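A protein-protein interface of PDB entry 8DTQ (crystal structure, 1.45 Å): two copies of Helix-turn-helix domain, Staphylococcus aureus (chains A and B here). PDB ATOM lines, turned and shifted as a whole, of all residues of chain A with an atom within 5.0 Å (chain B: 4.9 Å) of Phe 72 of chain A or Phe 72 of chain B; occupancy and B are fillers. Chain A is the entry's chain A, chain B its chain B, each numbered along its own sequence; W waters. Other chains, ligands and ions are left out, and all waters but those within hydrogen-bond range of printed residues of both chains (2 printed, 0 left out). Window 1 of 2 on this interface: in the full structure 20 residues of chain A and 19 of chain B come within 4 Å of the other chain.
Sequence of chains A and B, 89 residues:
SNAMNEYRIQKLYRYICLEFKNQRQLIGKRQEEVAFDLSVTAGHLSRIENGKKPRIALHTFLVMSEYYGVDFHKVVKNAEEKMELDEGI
OD1 of Asp 71 of chain A sits close to OE2 of Glu 80 of chain B (2.5 Å).
ND1 of His 73 of chain A lies within hydrogen-bond range of OE1 of Glu 80 of chain B (2.8 Å).
The side-chain carboxylate (OE2) of Glu 80 of chain A is in hydrogen-bond range of the backbone NH (N) of Phe 72 of chain B, at 3.3 Å.
A ring nitrogen (ND1) of His 73 of chain B sits at hydrogen-bond distance from the side-chain carboxylate (OE1) of Glu 80 of chain A (2.5 Å).
N of Leu 58 of chain A lies close to N of Leu 58 of chain B (3.5 Å).
Phe 72 of chain B touches its own counterpart, Phe 72 of chain A.
His 73 of chain B touches its own counterpart, His 73 of chain A.
His 73 of chain A touches Val 76 of chain B, and with the chains exchanged Val 76 of chain A touches His 73 of chain B.
Glu 80 of chain A touches Phe 72 of chain B, but with the chains exchanged Phe 72 of chain A does not touch Glu 80 of chain B (4.5 Å).
14 positions are printed for both chains.
Of the 14 pairs that touch across the chains among the printed residues, 11 have their exchanged pair printed and touching as well.
The backbone carbonyl oxygen (O) of Phe 61 of chain A is in hydrogen-bond range of the side-chain hydroxyl (OG) of Ser 65 of chain A, at 3.0 Å.
The side-chain carboxylate (OD1) of Asp 71 of chain A is in hydrogen-bond range of the backbone NH (N) of His 73 of chain A (2.9 Å).
The backbone carbonyl oxygen of Phe 61 of chain B sits at hydrogen-bond distance from the side-chain hydroxyl of Ser 65 of chain B.
Leu 58 of chain A touches Phe 61 of chain B.
Leu 58 of chain B touches Phe 61 of chain A.
Phe 72 of chain B touches Phe 72 of chain A.
His 73 of chain B touches His 73 of chain A.
CB of His 73 of chain A touches CG1 of Val 76 of chain B, 3.5 Å away.
Phe 72 of chain B touches Val 76 of chain A (CD2 to CG1, 3.8 Å).
Val 76 of chain A touches His 73 of chain B (CG1 to N, 3.5 Å).
N of Lys 77 of chain A touches CB of His 73 of chain B, at 3.6 Å.
OE2 of Glu 80 of chain A touches CB of Asp 71 of chain B, at 3.8 Å.
Of the printed residues of chain B, Phe 61 of chain A touches Leu 58 (3.5 Å).
Of the printed residues of chain B, Lys 77 of chain A touches His 73.
Printed residues of chain A within 4 Å of Phe 72 of chain B: Phe 72, Val 76 and Glu 80.
Printed residues of chain A within 4 Å of His 73 of chain B: His 73 (3.8 Å), Val 76 (3.5 Å), Lys 77 (3.6 Å) and Glu 80 (2.5 Å).
Val 75 of chain B touches none of the printed residues of chain A.
The nearest residue of chain B that does not touch Phe 72 of chain A is Val 76 of chain B (4.02 Å).
The nearest printed residue of chain A that does not touch Phe 72 of chain B is Leu 58 of chain A (4.4 Å).
The nearest printed residue of chain B that does not touch Phe 61 of chain A is Phe 72 of chain B (7.5 Å).
Water W1 bridges the side-chain carboxylate of Asp 71 of chain A and the side-chain carboxylate of Glu 80 of chain B.
Water W2 lies within hydrogen-bond range of OD1 of Asp 71 of chain B (2.8 Å) and OE2 of Glu 80 of chain A (3.1 Å).
Hydrophobic or aromatic side chains of chain B that line the printed part of chain A: Leu 58, Phe 61, Phe 72, His 73 and Val 76.
Along chain B the printed residues that touch a printed residue of chain A span positions 58 to 80.
Of the 15 printed residues of chain A, 8 touch a printed residue of chain B.
Hydrophobic or aromatic side chains of chain A that line the printed part of chain B: Leu 58, Phe 61, Phe 72, His 73 and Val 76.
Along chain A the printed residues that touch a printed residue of chain B span positions 58 to 80.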
ATOM      1  N   ILE A  16     -15.691  26.995  -4.739  1.00  0.00           N
ATOM      2  CA  ILE A  16     -14.968  26.023  -5.563  1.00  0.00           C
ATOM      3  C   ILE A  16     -15.894  25.441  -6.632  1.00  0.00           C
ATOM      4  O   ILE A  16     -15.536  25.354  -7.813  1.00  0.00           O
ATOM      5  CB  ILE A  16     -14.320  24.928  -4.687  1.00  0.00           C
ATOM      6  CG1 ILE A  16     -13.142  25.518  -3.866  1.00  0.00           C
ATOM      7  CG2 ILE A  16     -13.825  23.794  -5.564  1.00  0.00           C
ATOM      8  CD1 ILE A  16     -12.646  24.612  -2.712  1.00  0.00           C
ATOM      9  N   PHE A  20     -15.851  25.844 -11.063  1.00  0.00           N
ATOM     10  CA  PHE A  20     -15.997  24.894 -12.168  1.00  0.00           C
ATOM     11  C   PHE A  20     -17.033  25.358 -13.193  1.00  0.00           C
ATOM     12  O   PHE A  20     -16.868  25.120 -14.398  1.00  0.00           O
ATOM     13  CB  PHE A  20     -16.295  23.504 -11.622  1.00  0.00           C
ATOM     14  CG  PHE A  20     -15.070  22.816 -11.109  1.00  0.00           C
ATOM     15  CD1 PHE A  20     -14.106  22.343 -11.987  1.00  0.00           C
ATOM     16  CD2 PHE A  20     -14.847  22.708  -9.747  1.00  0.00           C
ATOM     17  CE1 PHE A  20     -12.955  21.727 -11.506  1.00  0.00           C
ATOM     18  CE2 PHE A  20     -13.701  22.107  -9.266  1.00  0.00           C
ATOM     19  CZ  PHE A  20     -12.760  21.603 -10.147  1.00  0.00           C
ATOM     20  N   LEU A  58     -13.872  14.712  -3.161  1.00  0.00           N
ATOM     21  CA  LEU A  58     -12.736  15.403  -3.763  1.00  0.00           C
ATOM     22  C   LEU A  58     -12.400  14.811  -5.125  1.00  0.00           C
ATOM     23  O   LEU A  58     -12.071  15.545  -6.063  1.00  0.00           O
ATOM     24  CB  LEU A  58     -11.515  15.358  -2.835  1.00  0.00           C
ATOM     25  CG  LEU A  58     -10.186  15.886  -3.421  1.00  0.00           C
ATOM     26  CD1 LEU A  58     -10.274  17.370  -3.839  1.00  0.00           C
ATOM     27  CD2 LEU A  58      -9.023  15.673  -2.448  1.00  0.00           C
ATOM     28  N   PHE A  61     -13.946  16.524  -8.097  1.00  0.00           N
ATOM     29  CA  PHE A  61     -13.319  17.773  -8.499  1.00  0.00           C
ATOM     30  C   PHE A  61     -11.986  17.546  -9.201  1.00  0.00           C
ATOM     31  O   PHE A  61     -11.648  18.297 -10.124  1.00  0.00           O
ATOM     32  CB  PHE A  61     -13.186  18.691  -7.287  1.00  0.00           C
ATOM     33  CG  PHE A  61     -14.523  19.039  -6.659  1.00  0.00           C
ATOM     34  CD1 PHE A  61     -14.906  18.464  -5.462  1.00  0.00           C
ATOM     35  CD2 PHE A  61     -15.403  19.897  -7.298  1.00  0.00           C
ATOM     36  CE1 PHE A  61     -16.136  18.758  -4.893  1.00  0.00           C
ATOM     37  CE2 PHE A  61     -16.642  20.209  -6.736  1.00  0.00           C
ATOM     38  CZ  PHE A  61     -17.003  19.652  -5.530  1.00  0.00           C
ATOM     39  N   LEU A  62     -11.231  16.516  -8.804  1.00  0.00           N
ATOM     40  CA  LEU A  62     -10.003  16.201  -9.532  1.00  0.00           C
ATOM     41  C   LEU A  62     -10.310  15.731 -10.947  1.00  0.00           C
ATOM     42  O   LEU A  62      -9.611  16.110 -11.895  1.00  0.00           O
ATOM     43  CB  LEU A  62      -9.182  15.150  -8.780  1.00  0.00           C
ATOM     44  CG  LEU A  62      -8.725  15.610  -7.399  1.00  0.00           C
ATOM     45  CD1 LEU A  62      -7.876  14.533  -6.739  1.00  0.00           C
ATOM     46  CD2 LEU A  62      -7.970  16.926  -7.494  1.00  0.00           C
ATOM     47  N   SER A  65     -11.216  18.792 -12.936  1.00  0.00           N
ATOM     48  CA  SER A  65     -10.049  19.617 -13.245  1.00  0.00           C
ATOM     49  C   SER A  65      -9.291  19.061 -14.439  1.00  0.00           C
ATOM     50  O   SER A  65      -8.874  19.811 -15.331  1.00  0.00           O
ATOM     51  CB  SER A  65      -9.108  19.688 -12.044  1.00  0.00           C
ATOM     52  OG  SER A  65      -9.663  20.420 -10.981  1.00  0.00           O
ATOM     53  N   VAL A  70      -7.481  22.317 -16.290  1.00  0.00           N
ATOM     54  CA  VAL A  70      -7.113  23.349 -15.333  1.00  0.00           C
ATOM     55  C   VAL A  70      -6.559  22.687 -14.074  1.00  0.00           C
ATOM     56  O   VAL A  70      -7.063  21.649 -13.628  1.00  0.00           O
ATOM     57  CB  VAL A  70      -8.314  24.268 -15.012  1.00  0.00           C
ATOM     58  CG1 VAL A  70      -9.449  23.494 -14.339  1.00  0.00           C
ATOM     59  CG2 VAL A  70      -7.872  25.466 -14.175  1.00  0.00           C
ATOM     60  N   ASP A  71      -5.474  23.252 -13.546  1.00  0.00           N
ATOM     61  CA  ASP A  71      -4.875  22.745 -12.319  1.00  0.00           C
ATOM     62  C   ASP A  71      -5.802  22.986 -11.132  1.00  0.00           C
ATOM     63  O   ASP A  71      -6.218  24.121 -10.881  1.00  0.00           O
ATOM     64  CB  ASP A  71      -3.545  23.464 -12.094  1.00  0.00           C
ATOM     65  CG  ASP A  71      -2.652  22.751 -11.104  1.00  0.00           C
ATOM     66  OD1 ASP A  71      -3.135  22.388 -10.014  1.00  0.00           O
ATOM     67  OD2 ASP A  71      -1.462  22.541 -11.436  1.00  0.00           O
ATOM     68  N   PHE A  72      -6.078  21.935 -10.353  1.00  0.00           N
ATOM     69  CA  PHE A  72      -6.977  22.100  -9.214  1.00  0.00           C
ATOM     70  C   PHE A  72      -6.454  23.127  -8.207  1.00  0.00           C
ATOM     71  O   PHE A  72      -7.254  23.828  -7.573  1.00  0.00           O
ATOM     72  CB  PHE A  72      -7.253  20.753  -8.546  1.00  0.00           C
ATOM     73  CG  PHE A  72      -8.302  20.801  -7.457  1.00  0.00           C
ATOM     74  CD1 PHE A  72      -9.582  21.280  -7.702  1.00  0.00           C
ATOM     75  CD2 PHE A  72      -8.007  20.340  -6.184  1.00  0.00           C
ATOM     76  CE1 PHE A  72     -10.542  21.296  -6.692  1.00  0.00           C
ATOM     77  CE2 PHE A  72      -8.941  20.353  -5.178  1.00  0.00           C
ATOM     78  CZ  PHE A  72     -10.222  20.823  -5.423  1.00  0.00           C
ATOM     79  N   HIS A  73      -5.133  23.259  -8.039  1.00  0.00           N
ATOM     80  CA  HIS A  73      -4.706  24.287  -7.085  1.00  0.00           C
ATOM     81  C   HIS A  73      -5.072  25.693  -7.537  1.00  0.00           C
ATOM     82  O   HIS A  73      -5.340  26.553  -6.693  1.00  0.00           O
ATOM     83  CB  HIS A  73      -3.250  24.148  -6.628  1.00  0.00           C
ATOM     84  CG  HIS A  73      -2.281  24.989  -7.387  1.00  0.00           C
ATOM     85  ND1 HIS A  73      -1.496  24.477  -8.401  1.00  0.00           N
ATOM     86  CD2 HIS A  73      -1.958  26.300  -7.287  1.00  0.00           C
ATOM     87  CE1 HIS A  73      -0.726  25.436  -8.885  1.00  0.00           C
ATOM     88  NE2 HIS A  73      -0.991  26.552  -8.231  1.00  0.00           N
ATOM     89  N   LYS A  74      -5.104  25.943  -8.845  1.00  0.00           N
ATOM     90  CA  LYS A  74      -5.530  27.253  -9.318  1.00  0.00           C
ATOM     91  C   LYS A  74      -7.032  27.427  -9.142  1.00  0.00           C
ATOM     92  O   LYS A  74      -7.502  28.519  -8.808  1.00  0.00           O
ATOM     93  CB  LYS A  74      -5.165  27.422 -10.788  1.00  0.00           C
ATOM     94  CG  LYS A  74      -5.654  28.732 -11.398  1.00  0.00           C
ATOM     95  CD  LYS A  74      -5.139  28.895 -12.822  1.00  0.00           C
ATOM     96  CE  LYS A  74      -6.278  28.957 -13.818  1.00  0.00           C
ATOM     97  NZ  LYS A  74      -7.002  30.261 -13.735  1.00  0.00           N
ATOM     98  N   VAL A  75      -7.804  26.357  -9.358  1.00  0.00           N
ATOM     99  CA  VAL A  75      -9.245  26.426  -9.115  1.00  0.00           C
ATOM    100  C   VAL A  75      -9.511  26.851  -7.678  1.00  0.00           C
ATOM    101  O   VAL A  75     -10.314  27.761  -7.416  1.00  0.00           O
ATOM    102  CB  VAL A  75      -9.910  25.067  -9.412  1.00  0.00           C
ATOM    103  CG1 VAL A  75     -11.361  25.066  -8.945  1.00  0.00           C
ATOM    104  CG2 VAL A  75      -9.813  24.707 -10.887  1.00  0.00           C
ATOM    105  N   VAL A  76      -8.850  26.182  -6.726  1.00  0.00           N
ATOM    106  CA  VAL A  76      -9.060  26.466  -5.311  1.00  0.00           C
ATOM    107  C   VAL A  76      -8.579  27.868  -4.972  1.00  0.00           C
ATOM    108  O   VAL A  76      -9.254  28.616  -4.251  1.00  0.00           O
ATOM    109  CB  VAL A  76      -8.394  25.393  -4.431  1.00  0.00           C
ATOM    110  CG1 VAL A  76      -8.560  25.751  -2.982  1.00  0.00           C
ATOM    111  CG2 VAL A  76      -9.000  24.031  -4.733  1.00  0.00           C
ATOM    112  N   LYS A  77      -7.414  28.258  -5.493  1.00  0.00           N
ATOM    113  CA  LYS A  77      -6.906  29.596  -5.209  1.00  0.00           C
ATOM    114  C   LYS A  77      -7.861  30.659  -5.743  1.00  0.00           C
ATOM    115  O   LYS A  77      -8.132  31.668  -5.068  1.00  0.00           O
ATOM    116  CB  LYS A  77      -5.499  29.781  -5.792  1.00  0.00           C
ATOM    117  CG  LYS A  77      -4.799  31.017  -5.262  1.00  0.00           C
ATOM    118  CD  LYS A  77      -3.358  31.136  -5.774  1.00  0.00           C
ATOM    119  CE  LYS A  77      -2.608  32.254  -5.084  1.00  0.00           C
ATOM    120  NZ  LYS A  77      -1.204  32.328  -5.603  1.00  0.00           N
ATOM    121  N   GLU A  80     -10.780  30.848  -3.305  1.00  0.00           N
ATOM    122  CA  GLU A  80     -10.444  31.533  -2.061  1.00  0.00           C
ATOM    123  C   GLU A  80     -10.387  33.037  -2.275  1.00  0.00           C
ATOM    124  O   GLU A  80     -10.904  33.818  -1.457  1.00  0.00           O
ATOM    125  CB  GLU A  80      -9.090  31.044  -1.541  1.00  0.00           C
ATOM    126  CG  GLU A  80      -9.029  29.571  -1.131  1.00  0.00           C
ATOM    127  CD  GLU A  80      -7.609  29.088  -0.913  1.00  0.00           C
ATOM    128  OE1 GLU A  80      -6.659  29.874  -1.163  1.00  0.00           O
ATOM    129  OE2 GLU A  80      -7.441  27.926  -0.493  1.00  0.00           O
ATOM    130  N   ILE B  16      -2.440  14.558  -1.646  1.00  0.00           N
ATOM    131  CA  ILE B  16      -3.184  15.500  -0.811  1.00  0.00           C
ATOM    132  C   ILE B  16      -3.409  14.914   0.576  1.00  0.00           C
ATOM    133  O   ILE B  16      -3.218  15.592   1.594  1.00  0.00           O
ATOM    134  CB  ILE B  16      -4.497  15.905  -1.505  1.00  0.00           C
ATOM    135  CG1 ILE B  16      -4.205  16.780  -2.730  1.00  0.00           C
ATOM    136  CG2 ILE B  16      -5.432  16.623  -0.543  1.00  0.00           C
ATOM    137  CD1 ILE B  16      -5.417  16.956  -3.681  1.00  0.00           C
ATOM    138  N   PHE B  20      -1.846  16.212   4.299  1.00  0.00           N
ATOM    139  CA  PHE B  20      -2.478  16.395   5.601  1.00  0.00           C
ATOM    140  C   PHE B  20      -1.780  15.589   6.686  1.00  0.00           C
ATOM    141  O   PHE B  20      -1.671  16.056   7.825  1.00  0.00           O
ATOM    142  CB  PHE B  20      -3.968  16.084   5.552  1.00  0.00           C
ATOM    143  CG  PHE B  20      -4.761  17.204   4.970  1.00  0.00           C
ATOM    144  CD1 PHE B  20      -4.868  18.413   5.654  1.00  0.00           C
ATOM    145  CD2 PHE B  20      -5.379  17.080   3.734  1.00  0.00           C
ATOM    146  CE1 PHE B  20      -5.604  19.479   5.118  1.00  0.00           C
ATOM    147  CE2 PHE B  20      -6.112  18.141   3.196  1.00  0.00           C
ATOM    148  CZ  PHE B  20      -6.225  19.331   3.891  1.00  0.00           C
ATOM    149  N   LEU B  58     -14.893  16.581  -0.416  1.00  0.00           N
ATOM    150  CA  LEU B  58     -14.116  17.819  -0.379  1.00  0.00           C
ATOM    151  C   LEU B  58     -14.319  18.539   0.951  1.00  0.00           C
ATOM    152  O   LEU B  58     -13.368  19.072   1.525  1.00  0.00           O
ATOM    153  CB  LEU B  58     -14.476  18.716  -1.568  1.00  0.00           C
ATOM    154  CG  LEU B  58     -13.869  20.124  -1.550  1.00  0.00           C
ATOM    155  CD1 LEU B  58     -12.333  20.053  -1.513  1.00  0.00           C
ATOM    156  CD2 LEU B  58     -14.336  20.901  -2.767  1.00  0.00           C
ATOM    157  N   PHE B  61     -11.799  17.678   3.601  1.00  0.00           N
ATOM    158  CA  PHE B  61     -10.494  18.292   3.391  1.00  0.00           C
ATOM    159  C   PHE B  61     -10.515  19.771   3.728  1.00  0.00           C
ATOM    160  O   PHE B  61      -9.522  20.297   4.248  1.00  0.00           O
ATOM    161  CB  PHE B  61     -10.009  18.031   1.966  1.00  0.00           C
ATOM    162  CG  PHE B  61      -9.771  16.569   1.686  1.00  0.00           C
ATOM    163  CD1 PHE B  61     -10.661  15.831   0.930  1.00  0.00           C
ATOM    164  CD2 PHE B  61      -8.675  15.934   2.234  1.00  0.00           C
ATOM    165  CE1 PHE B  61     -10.445  14.483   0.691  1.00  0.00           C
ATOM    166  CE2 PHE B  61      -8.437  14.578   2.004  1.00  0.00           C
ATOM    167  CZ  PHE B  61      -9.334  13.847   1.244  1.00  0.00           C
ATOM    168  N   LEU B  62     -11.636  20.454   3.480  1.00  0.00           N
ATOM    169  CA  LEU B  62     -11.739  21.855   3.883  1.00  0.00           C
ATOM    170  C   LEU B  62     -11.776  22.011   5.403  1.00  0.00           C
ATOM    171  O   LEU B  62     -11.210  22.977   5.948  1.00  0.00           O
ATOM    172  CB  LEU B  62     -12.944  22.501   3.212  1.00  0.00           C
ATOM    173  CG  LEU B  62     -12.906  22.533   1.682  1.00  0.00           C
ATOM    174  CD1 LEU B  62     -14.161  23.199   1.131  1.00  0.00           C
ATOM    175  CD2 LEU B  62     -11.669  23.306   1.196  1.00  0.00           C
ATOM    176  N   SER B  65      -8.188  21.646   6.488  1.00  0.00           N
ATOM    177  CA  SER B  65      -7.407  22.854   6.176  1.00  0.00           C
ATOM    178  C   SER B  65      -7.689  23.945   7.201  1.00  0.00           C
ATOM    179  O   SER B  65      -6.784  24.656   7.642  1.00  0.00           O
ATOM    180  CB  SER B  65      -7.756  23.380   4.784  1.00  0.00           C
ATOM    181  OG  SER B  65      -7.284  22.537   3.755  1.00  0.00           O
ATOM    182  N   VAL B  70      -4.053  26.148   7.292  1.00  0.00           N
ATOM    183  CA  VAL B  70      -3.321  26.236   6.036  1.00  0.00           C
ATOM    184  C   VAL B  70      -4.342  26.312   4.909  1.00  0.00           C
ATOM    185  O   VAL B  70      -5.292  25.527   4.884  1.00  0.00           O
ATOM    186  CB  VAL B  70      -2.388  25.023   5.863  1.00  0.00           C
ATOM    187  CG1 VAL B  70      -1.689  25.054   4.499  1.00  0.00           C
ATOM    188  CG2 VAL B  70      -1.355  24.991   6.983  1.00  0.00           C
ATOM    189  N   ASP B  71      -4.125  27.219   3.959  1.00  0.00           N
ATOM    190  CA  ASP B  71      -5.048  27.378   2.838  1.00  0.00           C
ATOM    191  C   ASP B  71      -5.114  26.089   2.048  1.00  0.00           C
ATOM    192  O   ASP B  71      -4.080  25.477   1.761  1.00  0.00           O
ATOM    193  CB  ASP B  71      -4.550  28.462   1.869  1.00  0.00           C
ATOM    194  CG  ASP B  71      -4.668  29.863   2.419  1.00  0.00           C
ATOM    195  OD1 ASP B  71      -5.594  30.131   3.212  1.00  0.00           O
ATOM    196  OD2 ASP B  71      -3.845  30.718   2.016  1.00  0.00           O
ATOM    197  N   PHE B  72      -6.323  25.655   1.701  1.00  0.00           N
ATOM    198  CA  PHE B  72      -6.415  24.420   0.932  1.00  0.00           C
ATOM    199  C   PHE B  72      -5.679  24.517  -0.402  1.00  0.00           C
ATOM    200  O   PHE B  72      -5.091  23.532  -0.851  1.00  0.00           O
ATOM    201  CB  PHE B  72      -7.874  24.007   0.747  1.00  0.00           C
ATOM    202  CG  PHE B  72      -8.036  22.647   0.107  1.00  0.00           C
ATOM    203  CD1 PHE B  72      -7.402  21.529   0.649  1.00  0.00           C
ATOM    204  CD2 PHE B  72      -8.823  22.488  -1.028  1.00  0.00           C
ATOM    205  CE1 PHE B  72      -7.561  20.282   0.075  1.00  0.00           C
ATOM    206  CE2 PHE B  72      -8.985  21.238  -1.617  1.00  0.00           C
ATOM    207  CZ  PHE B  72      -8.339  20.126  -1.062  1.00  0.00           C
ATOM    208  N   HIS B  73      -5.626  25.697  -1.031  1.00  0.00           N
ATOM    209  CA  HIS B  73      -4.866  25.773  -2.278  1.00  0.00           C
ATOM    210  C   HIS B  73      -3.386  25.492  -2.039  1.00  0.00           C
ATOM    211  O   HIS B  73      -2.724  24.902  -2.894  1.00  0.00           O
ATOM    212  CB  HIS B  73      -5.072  27.127  -2.977  1.00  0.00           C
ATOM    213  CG  HIS B  73      -4.056  28.164  -2.608  1.00  0.00           C
ATOM    214  ND1 HIS B  73      -4.297  29.107  -1.634  1.00  0.00           N
ATOM    215  CD2 HIS B  73      -2.814  28.422  -3.088  1.00  0.00           C
ATOM    216  CE1 HIS B  73      -3.243  29.893  -1.516  1.00  0.00           C
ATOM    217  NE2 HIS B  73      -2.326  29.495  -2.384  1.00  0.00           N
ATOM    218  N   LYS B  74      -2.871  25.858  -0.864  1.00  0.00           N
ATOM    219  CA  LYS B  74      -1.474  25.571  -0.529  1.00  0.00           C
ATOM    220  C   LYS B  74      -1.259  24.081  -0.239  1.00  0.00           C
ATOM    221  O   LYS B  74      -0.217  23.512  -0.603  1.00  0.00           O
ATOM    222  CB  LYS B  74      -1.071  26.404   0.679  1.00  0.00           C
ATOM    223  CG  LYS B  74       0.356  26.182   1.061  1.00  0.00           C
ATOM    224  CD  LYS B  74       1.233  26.803  -0.011  1.00  0.00           C
ATOM    225  CE  LYS B  74       2.714  26.721   0.355  1.00  0.00           C
ATOM    226  NZ  LYS B  74       3.604  27.457  -0.604  1.00  0.00           N
ATOM    227  N   VAL B  75      -2.226  23.429   0.414  1.00  0.00           N
ATOM    228  CA  VAL B  75      -2.175  21.971   0.579  1.00  0.00           C
ATOM    229  C   VAL B  75      -2.064  21.293  -0.785  1.00  0.00           C
ATOM    230  O   VAL B  75      -1.244  20.385  -0.991  1.00  0.00           O
ATOM    231  CB  VAL B  75      -3.419  21.482   1.352  1.00  0.00           C
ATOM    232  CG1 VAL B  75      -3.537  19.946   1.300  1.00  0.00           C
ATOM    233  CG2 VAL B  75      -3.399  21.968   2.795  1.00  0.00           C
ATOM    234  N   VAL B  76      -2.908  21.715  -1.736  1.00  0.00           N
ATOM    235  CA  VAL B  76      -2.911  21.106  -3.065  1.00  0.00           C
ATOM    236  C   VAL B  76      -1.596  21.378  -3.790  1.00  0.00           C
ATOM    237  O   VAL B  76      -1.002  20.473  -4.386  1.00  0.00           O
ATOM    238  CB  VAL B  76      -4.117  21.606  -3.889  1.00  0.00           C
ATOM    239  CG1 VAL B  76      -4.045  21.040  -5.288  1.00  0.00           C
ATOM    240  CG2 VAL B  76      -5.447  21.231  -3.212  1.00  0.00           C
ATOM    241  N   GLU B  80       1.176  18.643  -5.068  1.00  0.00           N
ATOM    242  CA  GLU B  80       1.678  18.566  -6.432  1.00  0.00           C
ATOM    243  C   GLU B  80       3.196  18.633  -6.457  1.00  0.00           C
ATOM    244  O   GLU B  80       3.845  17.882  -7.189  1.00  0.00           O
ATOM    245  CB  GLU B  80       1.084  19.688  -7.280  1.00  0.00           C
ATOM    246  CG  GLU B  80      -0.416  19.515  -7.451  1.00  0.00           C
ATOM    247  CD  GLU B  80      -1.074  20.673  -8.152  1.00  0.00           C
ATOM    248  OE1 GLU B  80      -0.595  21.808  -7.991  1.00  0.00           O
ATOM    249  OE2 GLU B  80      -2.085  20.444  -8.840  1.00  0.00           O
HETATM  250  O   HOH W   1       0.613  20.904 -10.851  1.00  0.00           O
HETATM  251  O   HOH W   2      -8.118  29.473   2.136  1.00  0.00           O
